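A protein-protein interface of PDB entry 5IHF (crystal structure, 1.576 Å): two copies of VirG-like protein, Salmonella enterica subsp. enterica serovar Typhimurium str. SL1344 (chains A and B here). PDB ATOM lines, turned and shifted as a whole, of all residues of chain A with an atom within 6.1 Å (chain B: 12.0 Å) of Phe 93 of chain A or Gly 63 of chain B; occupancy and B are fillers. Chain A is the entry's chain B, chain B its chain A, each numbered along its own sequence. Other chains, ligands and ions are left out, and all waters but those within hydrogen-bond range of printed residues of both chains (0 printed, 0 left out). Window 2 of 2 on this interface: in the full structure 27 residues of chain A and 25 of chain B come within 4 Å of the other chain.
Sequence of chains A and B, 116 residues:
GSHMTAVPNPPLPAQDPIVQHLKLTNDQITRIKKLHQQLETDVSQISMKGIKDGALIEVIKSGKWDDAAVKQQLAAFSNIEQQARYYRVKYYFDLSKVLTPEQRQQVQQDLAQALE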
ATOM      1  N   ARG A  88      29.387  30.346 -11.409  1.00  0.00           N
ATOM      2  CA  ARG A  88      29.465  29.403 -10.301  1.00  0.00           C
ATOM      3  C   ARG A  88      29.055  28.005 -10.757  1.00  0.00           C
ATOM      4  O   ARG A  88      29.711  27.019 -10.415  1.00  0.00           O
ATOM      5  CB  ARG A  88      28.599  29.879  -9.135  1.00  0.00           C
ATOM      6  CG  ARG A  88      29.140  31.156  -8.520  1.00  0.00           C
ATOM      7  CD  ARG A  88      28.193  31.781  -7.511  1.00  0.00           C
ATOM      8  NE  ARG A  88      28.714  33.064  -7.048  1.00  0.00           N
ATOM      9  CZ  ARG A  88      28.000  33.975  -6.394  1.00  0.00           C
ATOM     10  NH1 ARG A  88      26.723  33.755  -6.122  1.00  0.00           N
ATOM     11  NH2 ARG A  88      28.565  35.113  -6.017  1.00  0.00           N
ATOM     12  N   VAL A  89      27.990  27.922 -11.549  1.00  0.00           N
ATOM     13  CA  VAL A  89      27.566  26.652 -12.127  1.00  0.00           C
ATOM     14  C   VAL A  89      28.663  26.095 -13.035  1.00  0.00           C
ATOM     15  O   VAL A  89      29.002  24.913 -12.955  1.00  0.00           O
ATOM     16  CB  VAL A  89      26.247  26.801 -12.924  1.00  0.00           C
ATOM     17  CG1 VAL A  89      25.905  25.519 -13.688  1.00  0.00           C
ATOM     18  CG2 VAL A  89      25.108  27.160 -11.990  1.00  0.00           C
ATOM     19  N   LYS A  90      29.225  26.940 -13.894  1.00  0.00           N
ATOM     20  CA  LYS A  90      30.255  26.487 -14.828  1.00  0.00           C
ATOM     21  C   LYS A  90      31.488  25.992 -14.069  1.00  0.00           C
ATOM     22  O   LYS A  90      32.152  25.055 -14.507  1.00  0.00           O
ATOM     23  CB  LYS A  90      30.638  27.603 -15.803  1.00  0.00           C
ATOM     24  CG  LYS A  90      31.578  27.170 -16.950  1.00  0.00           C
ATOM     25  CD  LYS A  90      31.952  28.359 -17.832  1.00  0.00           C
ATOM     26  CE  LYS A  90      33.064  28.049 -18.832  1.00  0.00           C
ATOM     27  NZ  LYS A  90      34.414  27.748 -18.215  1.00  0.00           N
ATOM     28  N   TYR A  91      31.780  26.607 -12.926  1.00  0.00           N
ATOM     29  CA  TYR A  91      32.909  26.196 -12.091  1.00  0.00           C
ATOM     30  C   TYR A  91      32.753  24.757 -11.619  1.00  0.00           C
ATOM     31  O   TYR A  91      33.671  23.946 -11.755  1.00  0.00           O
ATOM     32  CB  TYR A  91      33.047  27.133 -10.888  1.00  0.00           C
ATOM     33  CG  TYR A  91      33.980  26.646  -9.800  1.00  0.00           C
ATOM     34  CD1 TYR A  91      35.353  26.582 -10.009  1.00  0.00           C
ATOM     35  CD2 TYR A  91      33.489  26.277  -8.554  1.00  0.00           C
ATOM     36  CE1 TYR A  91      36.208  26.153  -9.015  1.00  0.00           C
ATOM     37  CE2 TYR A  91      34.337  25.849  -7.549  1.00  0.00           C
ATOM     38  CZ  TYR A  91      35.697  25.787  -7.786  1.00  0.00           C
ATOM     39  OH  TYR A  91      36.556  25.361  -6.797  1.00  0.00           O
ATOM     40  N   TYR A  92      31.590  24.433 -11.066  1.00  0.00           N
ATOM     41  CA  TYR A  92      31.365  23.079 -10.578  1.00  0.00           C
ATOM     42  C   TYR A  92      31.324  22.088 -11.740  1.00  0.00           C
ATOM     43  O   TYR A  92      31.760  20.942 -11.603  1.00  0.00           O
ATOM     44  CB  TYR A  92      30.086  23.023  -9.741  1.00  0.00           C
ATOM     45  CG  TYR A  92      30.304  23.577  -8.350  1.00  0.00           C
ATOM     46  CD1 TYR A  92      31.167  22.945  -7.465  1.00  0.00           C
ATOM     47  CD2 TYR A  92      29.671  24.739  -7.929  1.00  0.00           C
ATOM     48  CE1 TYR A  92      31.389  23.443  -6.199  1.00  0.00           C
ATOM     49  CE2 TYR A  92      29.885  25.247  -6.656  1.00  0.00           C
ATOM     50  CZ  TYR A  92      30.746  24.592  -5.799  1.00  0.00           C
ATOM     51  OH  TYR A  92      30.972  25.081  -4.532  1.00  0.00           O
ATOM     52  N   PHE A  93      30.829  22.539 -12.889  1.00  0.00           N
ATOM     53  CA  PHE A  93      30.842  21.724 -14.099  1.00  0.00           C
ATOM     54  C   PHE A  93      32.275  21.416 -14.522  1.00  0.00           C
ATOM     55  O   PHE A  93      32.620  20.261 -14.787  1.00  0.00           O
ATOM     56  CB  PHE A  93      30.093  22.438 -15.228  1.00  0.00           C
ATOM     57  CG  PHE A  93      30.137  21.717 -16.546  1.00  0.00           C
ATOM     58  CD1 PHE A  93      29.280  20.660 -16.804  1.00  0.00           C
ATOM     59  CD2 PHE A  93      31.023  22.110 -17.533  1.00  0.00           C
ATOM     60  CE1 PHE A  93      29.317  20.003 -18.019  1.00  0.00           C
ATOM     61  CE2 PHE A  93      31.063  21.455 -18.748  1.00  0.00           C
ATOM     62  CZ  PHE A  93      30.209  20.403 -18.989  1.00  0.00           C
ATOM     63  N   ASP A  94      33.110  22.450 -14.571  1.00  0.00           N
ATOM     64  CA  ASP A  94      34.503  22.293 -14.985  1.00  0.00           C
ATOM     65  C   ASP A  94      35.292  21.502 -13.949  1.00  0.00           C
ATOM     66  O   ASP A  94      36.142  20.676 -14.296  1.00  0.00           O
ATOM     67  CB  ASP A  94      35.157  23.660 -15.211  1.00  0.00           C
ATOM     68  CG  ASP A  94      34.622  24.369 -16.442  1.00  0.00           C
ATOM     69  OD1 ASP A  94      34.049  23.694 -17.321  1.00  0.00           O
ATOM     70  OD2 ASP A  94      34.786  25.604 -16.536  1.00  0.00           O
ATOM     71  N   LEU A  95      34.997  21.764 -12.683  1.00  0.00           N
ATOM     72  CA  LEU A  95      35.582  21.038 -11.567  1.00  0.00           C
ATOM     73  C   LEU A  95      35.351  19.537 -11.721  1.00  0.00           C
ATOM     74  O   LEU A  95      36.262  18.731 -11.529  1.00  0.00           O
ATOM     75  CB  LEU A  95      34.979  21.559 -10.259  1.00  0.00           C
ATOM     76  CG  LEU A  95      35.505  21.059  -8.919  1.00  0.00           C
ATOM     77  CD1 LEU A  95      35.332  22.159  -7.878  1.00  0.00           C
ATOM     78  CD2 LEU A  95      34.771  19.803  -8.490  1.00  0.00           C
ATOM     79  N   SER A  96      34.135  19.163 -12.097  1.00  0.00           N
ATOM     80  CA  SER A  96      33.767  17.754 -12.198  1.00  0.00           C
ATOM     81  C   SER A  96      34.582  17.000 -13.247  1.00  0.00           C
ATOM     82  O   SER A  96      34.730  15.778 -13.162  1.00  0.00           O
ATOM     83  CB  SER A  96      32.278  17.629 -12.517  1.00  0.00           C
ATOM     84  OG  SER A  96      31.498  18.119 -11.445  1.00  0.00           O
ATOM     85  N   LYS A  97      35.115  17.723 -14.227  1.00  0.00           N
ATOM     86  CA  LYS A  97      35.837  17.098 -15.332  1.00  0.00           C
ATOM     87  C   LYS A  97      37.172  16.488 -14.910  1.00  0.00           C
ATOM     88  O   LYS A  97      37.692  15.611 -15.603  1.00  0.00           O
ATOM     89  CB  LYS A  97      36.079  18.113 -16.455  1.00  0.00           C
ATOM     90  CG  LYS A  97      34.804  18.611 -17.118  1.00  0.00           C
ATOM     91  CD  LYS A  97      35.094  19.645 -18.197  1.00  0.00           C
ATOM     92  CE  LYS A  97      34.573  19.193 -19.553  1.00  0.00           C
ATOM     93  NZ  LYS A  97      34.625  20.272 -20.576  1.00  0.00           N
ATOM     94  N   LEU A 111      25.653  18.873  -4.474  1.00  0.00           N
ATOM     95  CA  LEU A 111      25.114  20.045  -5.160  1.00  0.00           C
ATOM     96  C   LEU A 111      23.595  19.978  -5.282  1.00  0.00           C
ATOM     97  O   LEU A 111      22.910  20.990  -5.129  1.00  0.00           O
ATOM     98  CB  LEU A 111      25.740  20.191  -6.549  1.00  0.00           C
ATOM     99  CG  LEU A 111      27.161  20.756  -6.617  1.00  0.00           C
ATOM    100  CD1 LEU A 111      27.623  20.811  -8.059  1.00  0.00           C
ATOM    101  CD2 LEU A 111      27.258  22.142  -5.986  1.00  0.00           C
ATOM    102  N   GLY B  54      17.680  21.278 -11.713  1.00  0.00           N
ATOM    103  CA  GLY B  54      17.255  20.685 -12.968  1.00  0.00           C
ATOM    104  C   GLY B  54      18.382  20.649 -13.981  1.00  0.00           C
ATOM    105  O   GLY B  54      19.214  19.742 -13.966  1.00  0.00           O
ATOM    106  N   ALA B  55      18.412  21.642 -14.863  1.00  0.00           N
ATOM    107  CA  ALA B  55      19.460  21.738 -15.870  1.00  0.00           C
ATOM    108  C   ALA B  55      20.826  21.920 -15.217  1.00  0.00           C
ATOM    109  O   ALA B  55      21.842  21.480 -15.754  1.00  0.00           O
ATOM    110  CB  ALA B  55      19.173  22.885 -16.823  1.00  0.00           C
ATOM    111  N   LEU B  56      20.845  22.568 -14.056  1.00  0.00           N
ATOM    112  CA  LEU B  56      22.090  22.799 -13.332  1.00  0.00           C
ATOM    113  C   LEU B  56      22.733  21.481 -12.901  1.00  0.00           C
ATOM    114  O   LEU B  56      23.956  21.354 -12.892  1.00  0.00           O
ATOM    115  CB  LEU B  56      21.842  23.686 -12.109  1.00  0.00           C
ATOM    116  CG  LEU B  56      21.140  25.028 -12.347  1.00  0.00           C
ATOM    117  CD1 LEU B  56      21.297  25.924 -11.125  1.00  0.00           C
ATOM    118  CD2 LEU B  56      21.653  25.732 -13.600  1.00  0.00           C
ATOM    119  N   ILE B  57      21.906  20.502 -12.545  1.00  0.00           N
ATOM    120  CA  ILE B  57      22.403  19.195 -12.124  1.00  0.00           C
ATOM    121  C   ILE B  57      22.675  18.309 -13.337  1.00  0.00           C
ATOM    122  O   ILE B  57      23.601  17.497 -13.330  1.00  0.00           O
ATOM    123  CB  ILE B  57      21.402  18.487 -11.181  1.00  0.00           C
ATOM    124  CG1 ILE B  57      21.153  19.332  -9.928  1.00  0.00           C
ATOM    125  CG2 ILE B  57      21.901  17.094 -10.790  1.00  0.00           C
ATOM    126  CD1 ILE B  57      22.393  19.584  -9.077  1.00  0.00           C
ATOM    127  N   GLU B  58      21.872  18.478 -14.382  1.00  0.00           N
ATOM    128  CA  GLU B  58      21.975  17.634 -15.565  1.00  0.00           C
ATOM    129  C   GLU B  58      23.312  17.822 -16.277  1.00  0.00           C
ATOM    130  O   GLU B  58      23.864  16.867 -16.817  1.00  0.00           O
ATOM    131  CB  GLU B  58      20.815  17.922 -16.523  1.00  0.00           C
ATOM    132  CG  GLU B  58      20.418  16.734 -17.406  1.00  0.00           C
ATOM    133  CD  GLU B  58      21.190  16.663 -18.714  1.00  0.00           C
ATOM    134  OE1 GLU B  58      21.600  17.722 -19.236  1.00  0.00           O
ATOM    135  OE2 GLU B  58      21.378  15.540 -19.225  1.00  0.00           O
ATOM    136  N   VAL B  59      23.840  19.044 -16.273  1.00  0.00           N
ATOM    137  CA  VAL B  59      25.122  19.298 -16.931  1.00  0.00           C
ATOM    138  C   VAL B  59      26.261  18.593 -16.195  1.00  0.00           C
ATOM    139  O   VAL B  59      27.212  18.127 -16.819  1.00  0.00           O
ATOM    140  CB  VAL B  59      25.437  20.812 -17.033  1.00  0.00           C
ATOM    141  CG1 VAL B  59      24.469  21.493 -17.986  1.00  0.00           C
ATOM    142  CG2 VAL B  59      25.401  21.474 -15.664  1.00  0.00           C
ATOM    143  N   ILE B  60      26.167  18.516 -14.871  1.00  0.00           N
ATOM    144  CA  ILE B  60      27.192  17.840 -14.082  1.00  0.00           C
ATOM    145  C   ILE B  60      27.115  16.339 -14.335  1.00  0.00           C
ATOM    146  O   ILE B  60      28.134  15.674 -14.532  1.00  0.00           O
ATOM    147  CB  ILE B  60      27.042  18.099 -12.561  1.00  0.00           C
ATOM    148  CG1 ILE B  60      26.797  19.583 -12.254  1.00  0.00           C
ATOM    149  CG2 ILE B  60      28.272  17.587 -11.816  1.00  0.00           C
ATOM    150  CD1 ILE B  60      28.006  20.486 -12.441  1.00  0.00           C
ATOM    151  N   LYS B  61      25.894  15.812 -14.328  1.00  0.00           N
ATOM    152  CA  LYS B  61      25.667  14.383 -14.527  1.00  0.00           C
ATOM    153  C   LYS B  61      26.067  13.935 -15.930  1.00  0.00           C
ATOM    154  O   LYS B  61      26.765  12.936 -16.094  1.00  0.00           O
ATOM    155  CB  LYS B  61      24.197  14.041 -14.272  1.00  0.00           C
ATOM    156  N   SER B  62      25.624  14.678 -16.939  1.00  0.00           N
ATOM    157  CA  SER B  62      25.875  14.313 -18.330  1.00  0.00           C
ATOM    158  C   SER B  62      27.293  14.655 -18.771  1.00  0.00           C
ATOM    159  O   SER B  62      27.839  14.024 -19.677  1.00  0.00           O
ATOM    160  CB  SER B  62      24.873  15.010 -19.252  1.00  0.00           C
ATOM    161  OG  SER B  62      24.955  16.417 -19.120  1.00  0.00           O
ATOM    162  N   GLY B  63      27.884  15.657 -18.131  1.00  0.00           N
ATOM    163  CA  GLY B  63      29.191  16.143 -18.529  1.00  0.00           C
ATOM    164  C   GLY B  63      29.115  16.951 -19.811  1.00  0.00           C
ATOM    165  O   GLY B  63      30.134  17.213 -20.449  1.00  0.00           O
ATOM    166  N   LYS B  64      27.898  17.343 -20.181  1.00  0.00           N
ATOM    167  CA  LYS B  64      27.662  18.140 -21.381  1.00  0.00           C
ATOM    168  C   LYS B  64      27.057  19.487 -21.007  1.00  0.00           C
ATOM    169  O   LYS B  64      25.962  19.551 -20.450  1.00  0.00           O
ATOM    170  CB  LYS B  64      26.734  17.399 -22.349  1.00  0.00           C
ATOM    171  N   TRP B  65      27.777  20.561 -21.313  1.00  0.00           N
ATOM    172  CA  TRP B  65      27.308  21.902 -20.996  1.00  0.00           C
ATOM    173  C   TRP B  65      26.143  22.297 -21.892  1.00  0.00           C
ATOM    174  O   TRP B  65      26.229  22.193 -23.118  1.00  0.00           O
ATOM    175  CB  TRP B  65      28.445  22.910 -21.142  1.00  0.00           C
ATOM    176  CG  TRP B  65      28.074  24.290 -20.711  1.00  0.00           C
ATOM    177  CD1 TRP B  65      27.890  25.378 -21.509  1.00  0.00           C
ATOM    178  CD2 TRP B  65      27.849  24.728 -19.368  1.00  0.00           C
ATOM    179  NE1 TRP B  65      27.563  26.474 -20.745  1.00  0.00           N
ATOM    180  CE2 TRP B  65      27.530  26.102 -19.427  1.00  0.00           C
ATOM    181  CE3 TRP B  65      27.886  24.100 -18.121  1.00  0.00           C
ATOM    182  CZ2 TRP B  65      27.251  26.850 -18.289  1.00  0.00           C
ATOM    183  CZ3 TRP B  65      27.606  24.841 -16.993  1.00  0.00           C
ATOM    184  CH2 TRP B  65      27.292  26.203 -17.083  1.00  0.00           C
ATOM    185  N   ASP B  66      25.055  22.742 -21.270  1.00  0.00           N
ATOM    186  CA  ASP B  66      23.900  23.256 -21.997  1.00  0.00           C
ATOM    187  C   ASP B  66      23.679  24.711 -21.598  1.00  0.00           C
ATOM    188  O   ASP B  66      22.961  25.010 -20.643  1.00  0.00           O
ATOM    189  CB  ASP B  66      22.657  22.413 -21.711  1.00  0.00           C
ATOM    190  CG  ASP B  66      21.515  22.712 -22.665  1.00  0.00           C
ATOM    191  OD1 ASP B  66      21.386  23.874 -23.106  1.00  0.00           O
ATOM    192  OD2 ASP B  66      20.746  21.780 -22.980  1.00  0.00           O
ATOM    193  N   ASP B  67      24.310  25.606 -22.349  1.00  0.00           N
ATOM    194  CA  ASP B  67      24.339  27.026 -22.025  1.00  0.00           C
ATOM    195  C   ASP B  67      22.949  27.642 -21.876  1.00  0.00           C
ATOM    196  O   ASP B  67      22.676  28.355 -20.908  1.00  0.00           O
ATOM    197  CB  ASP B  67      25.114  27.778 -23.103  1.00  0.00           C
ATOM    198  CG  ASP B  67      25.675  29.085 -22.606  1.00  0.00           C
ATOM    199  OD1 ASP B  67      26.677  29.047 -21.867  1.00  0.00           O
ATOM    200  OD2 ASP B  67      25.118  30.146 -22.956  1.00  0.00           O
ATOM    201  N   ALA B  68      22.076  27.376 -22.841  1.00  0.00           N
ATOM    202  CA  ALA B  68      20.747  27.973 -22.844  1.00  0.00           C
ATOM    203  C   ALA B  68      19.909  27.472 -21.669  1.00  0.00           C
ATOM    204  O   ALA B  68      19.172  28.241 -21.048  1.00  0.00           O
ATOM    205  CB  ALA B  68      20.044  27.681 -24.154  1.00  0.00           C
ATOM    206  N   ALA B  69      20.028  26.183 -21.372  1.00  0.00           N
ATOM    207  CA  ALA B  69      19.289  25.577 -20.271  1.00  0.00           C
ATOM    208  C   ALA B  69      19.728  26.167 -18.936  1.00  0.00           C
ATOM    209  O   ALA B  69      18.894  26.464 -18.076  1.00  0.00           O
ATOM    210  CB  ALA B  69      19.479  24.067 -20.273  1.00  0.00           C
ATOM    211  N   VAL B  70      21.036  26.336 -18.764  1.00  0.00           N
ATOM    212  CA  VAL B  70      21.566  26.922 -17.534  1.00  0.00           C
ATOM    213  C   VAL B  70      21.073  28.359 -17.376  1.00  0.00           C
ATOM    214  O   VAL B  70      20.589  28.741 -16.312  1.00  0.00           O
ATOM    215  CB  VAL B  70      23.112  26.879 -17.512  1.00  0.00           C
ATOM    216  CG1 VAL B  70      23.685  27.757 -16.397  1.00  0.00           C
ATOM    217  CG2 VAL B  70      23.585  25.446 -17.348  1.00  0.00           C
ATOM    218  N   LYS B  71      21.191  29.153 -18.436  1.00  0.00           N
ATOM    219  CA  LYS B  71      20.722  30.538 -18.399  1.00  0.00           C
ATOM    220  C   LYS B  71      19.222  30.632 -18.130  1.00  0.00           C
ATOM    221  O   LYS B  71      18.776  31.492 -17.367  1.00  0.00           O
ATOM    222  CB  LYS B  71      21.052  31.245 -19.712  1.00  0.00           C
ATOM    223  CG  LYS B  71      22.515  31.615 -19.856  1.00  0.00           C
ATOM    224  CD  LYS B  71      22.785  32.288 -21.186  1.00  0.00           C
ATOM    225  CE  LYS B  71      24.237  32.711 -21.310  1.00  0.00           C
ATOM    226  NZ  LYS B  71      24.521  33.295 -22.648  1.00  0.00           N
ATOM    227  N   LEU B  74      18.483  29.929 -14.459  1.00  0.00           N
ATOM    228  CA  LEU B  74      18.950  31.009 -13.601  1.00  0.00           C
ATOM    229  C   LEU B  74      18.070  32.245 -13.759  1.00  0.00           C
ATOM    230  O   LEU B  74      17.847  32.978 -12.796  1.00  0.00           O
ATOM    231  CB  LEU B  74      20.409  31.349 -13.905  1.00  0.00           C
ATOM    232  CG  LEU B  74      21.412  30.263 -13.514  1.00  0.00           C
ATOM    233  CD1 LEU B  74      22.799  30.647 -13.977  1.00  0.00           C
ATOM    234  CD2 LEU B  74      21.397  30.008 -12.009  1.00  0.00           C
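OG of Ser 62 of chain B lies close to N of Lys 64 of chain B. The indole nitrogen of Trp 65 of chain B lies within hydrogen-bond range of the side-chain carboxylate of Asp 67 of chain B (2.9 Å). The side-chain amino group (NZ) of Lys 90 of chain A lies within salt-bridge range of the side-chain carboxylate (OD2) of Asp 94 of chain A. The side-chain hydroxyl (OG) of Ser 96 of chain A is in hydrogen-bond range of the backbone carbonyl oxygen (O) of Tyr 92 of chain A (2.8 Å).
CG1 of Val 89 of chain A touches CH2 of Trp 65 of chain B, at 3.7 Å. Lys 90 of chain A touches Trp 65 of chain B (CA to CH2, 3.7 Å). Tyr 92 of chain A touches Ile 60 of chain B (C to CD1, 3.8 Å). Val 59 of chain B touches Phe 93 of chain A. Ile 60 of chain B touches Phe 93 of chain A. Phe 93 of chain A touches Gly 63 of chain B. Phe 93 of chain A touches Lys 64 of chain B. Phe 93 of chain A touches Trp 65 of chain B (CZ to N, 3.4 Å). Ile 60 of chain B touches Ser 96 of chain A (CG2 to OG, 3.3 Å).
Of chain B, only Trp 65 comes within 4 Å of Lys 90 of chain A. Tyr 91 of chain A touches none of the printed residues of chain B. Printed residues of chain B within 4 Å of Tyr 92 of chain A: Ile 60. Of the printed residues of chain B, Phe 93 of chain A touches Val 59 (3.1 Å), Ile 60 (3.5 Å), Gly 63 (3.5 Å), Lys 64 (3.7 Å) and Trp 65 (3.4 Å). No residue of chain B comes within 4 Å of Asp 94 of chain A. No residue of chain B comes within 4 Å of Leu 95 of chain A. Of chain B, only Ile 60 (3.3 Å) comes within 4 Å of Ser 96 of chain A. No residue of chain B comes within 4 Å of Lys 97 of chain A. Of the printed residues of chain A, Val 59 of chain B touches Phe 93. Of the printed residues of chain A, Ile 60 of chain B touches Tyr 92 (3.8 Å), Phe 93 (3.5 Å) and Ser 96 (3.3 Å). Printed residues of chain A within 4 Å of Gly 63 of chain B: Phe 93. The nearest printed residue of chain A that does not touch Ile 60 of chain B is Leu 111 of chain A (4.4 Å).
Hydrophobic or aromatic side chains of chain B within 4 Å of the printed part of chain A: Val 59, Ile 60 and Trp 65. Of the 11 printed residues of chain A, 5 touch a printed residue of chain B. Hydrophobic or aromatic side chains of chain A that line the printed part of chain B: Val 89 and Phe 93. Among the printed residues, 9 pairs touch across the chains. Among the printed residues, no Asp or Glu carboxylate lies within 4 Å of a Lys or Arg side-chain nitrogen of the other chain.
No position is printed for both chains.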
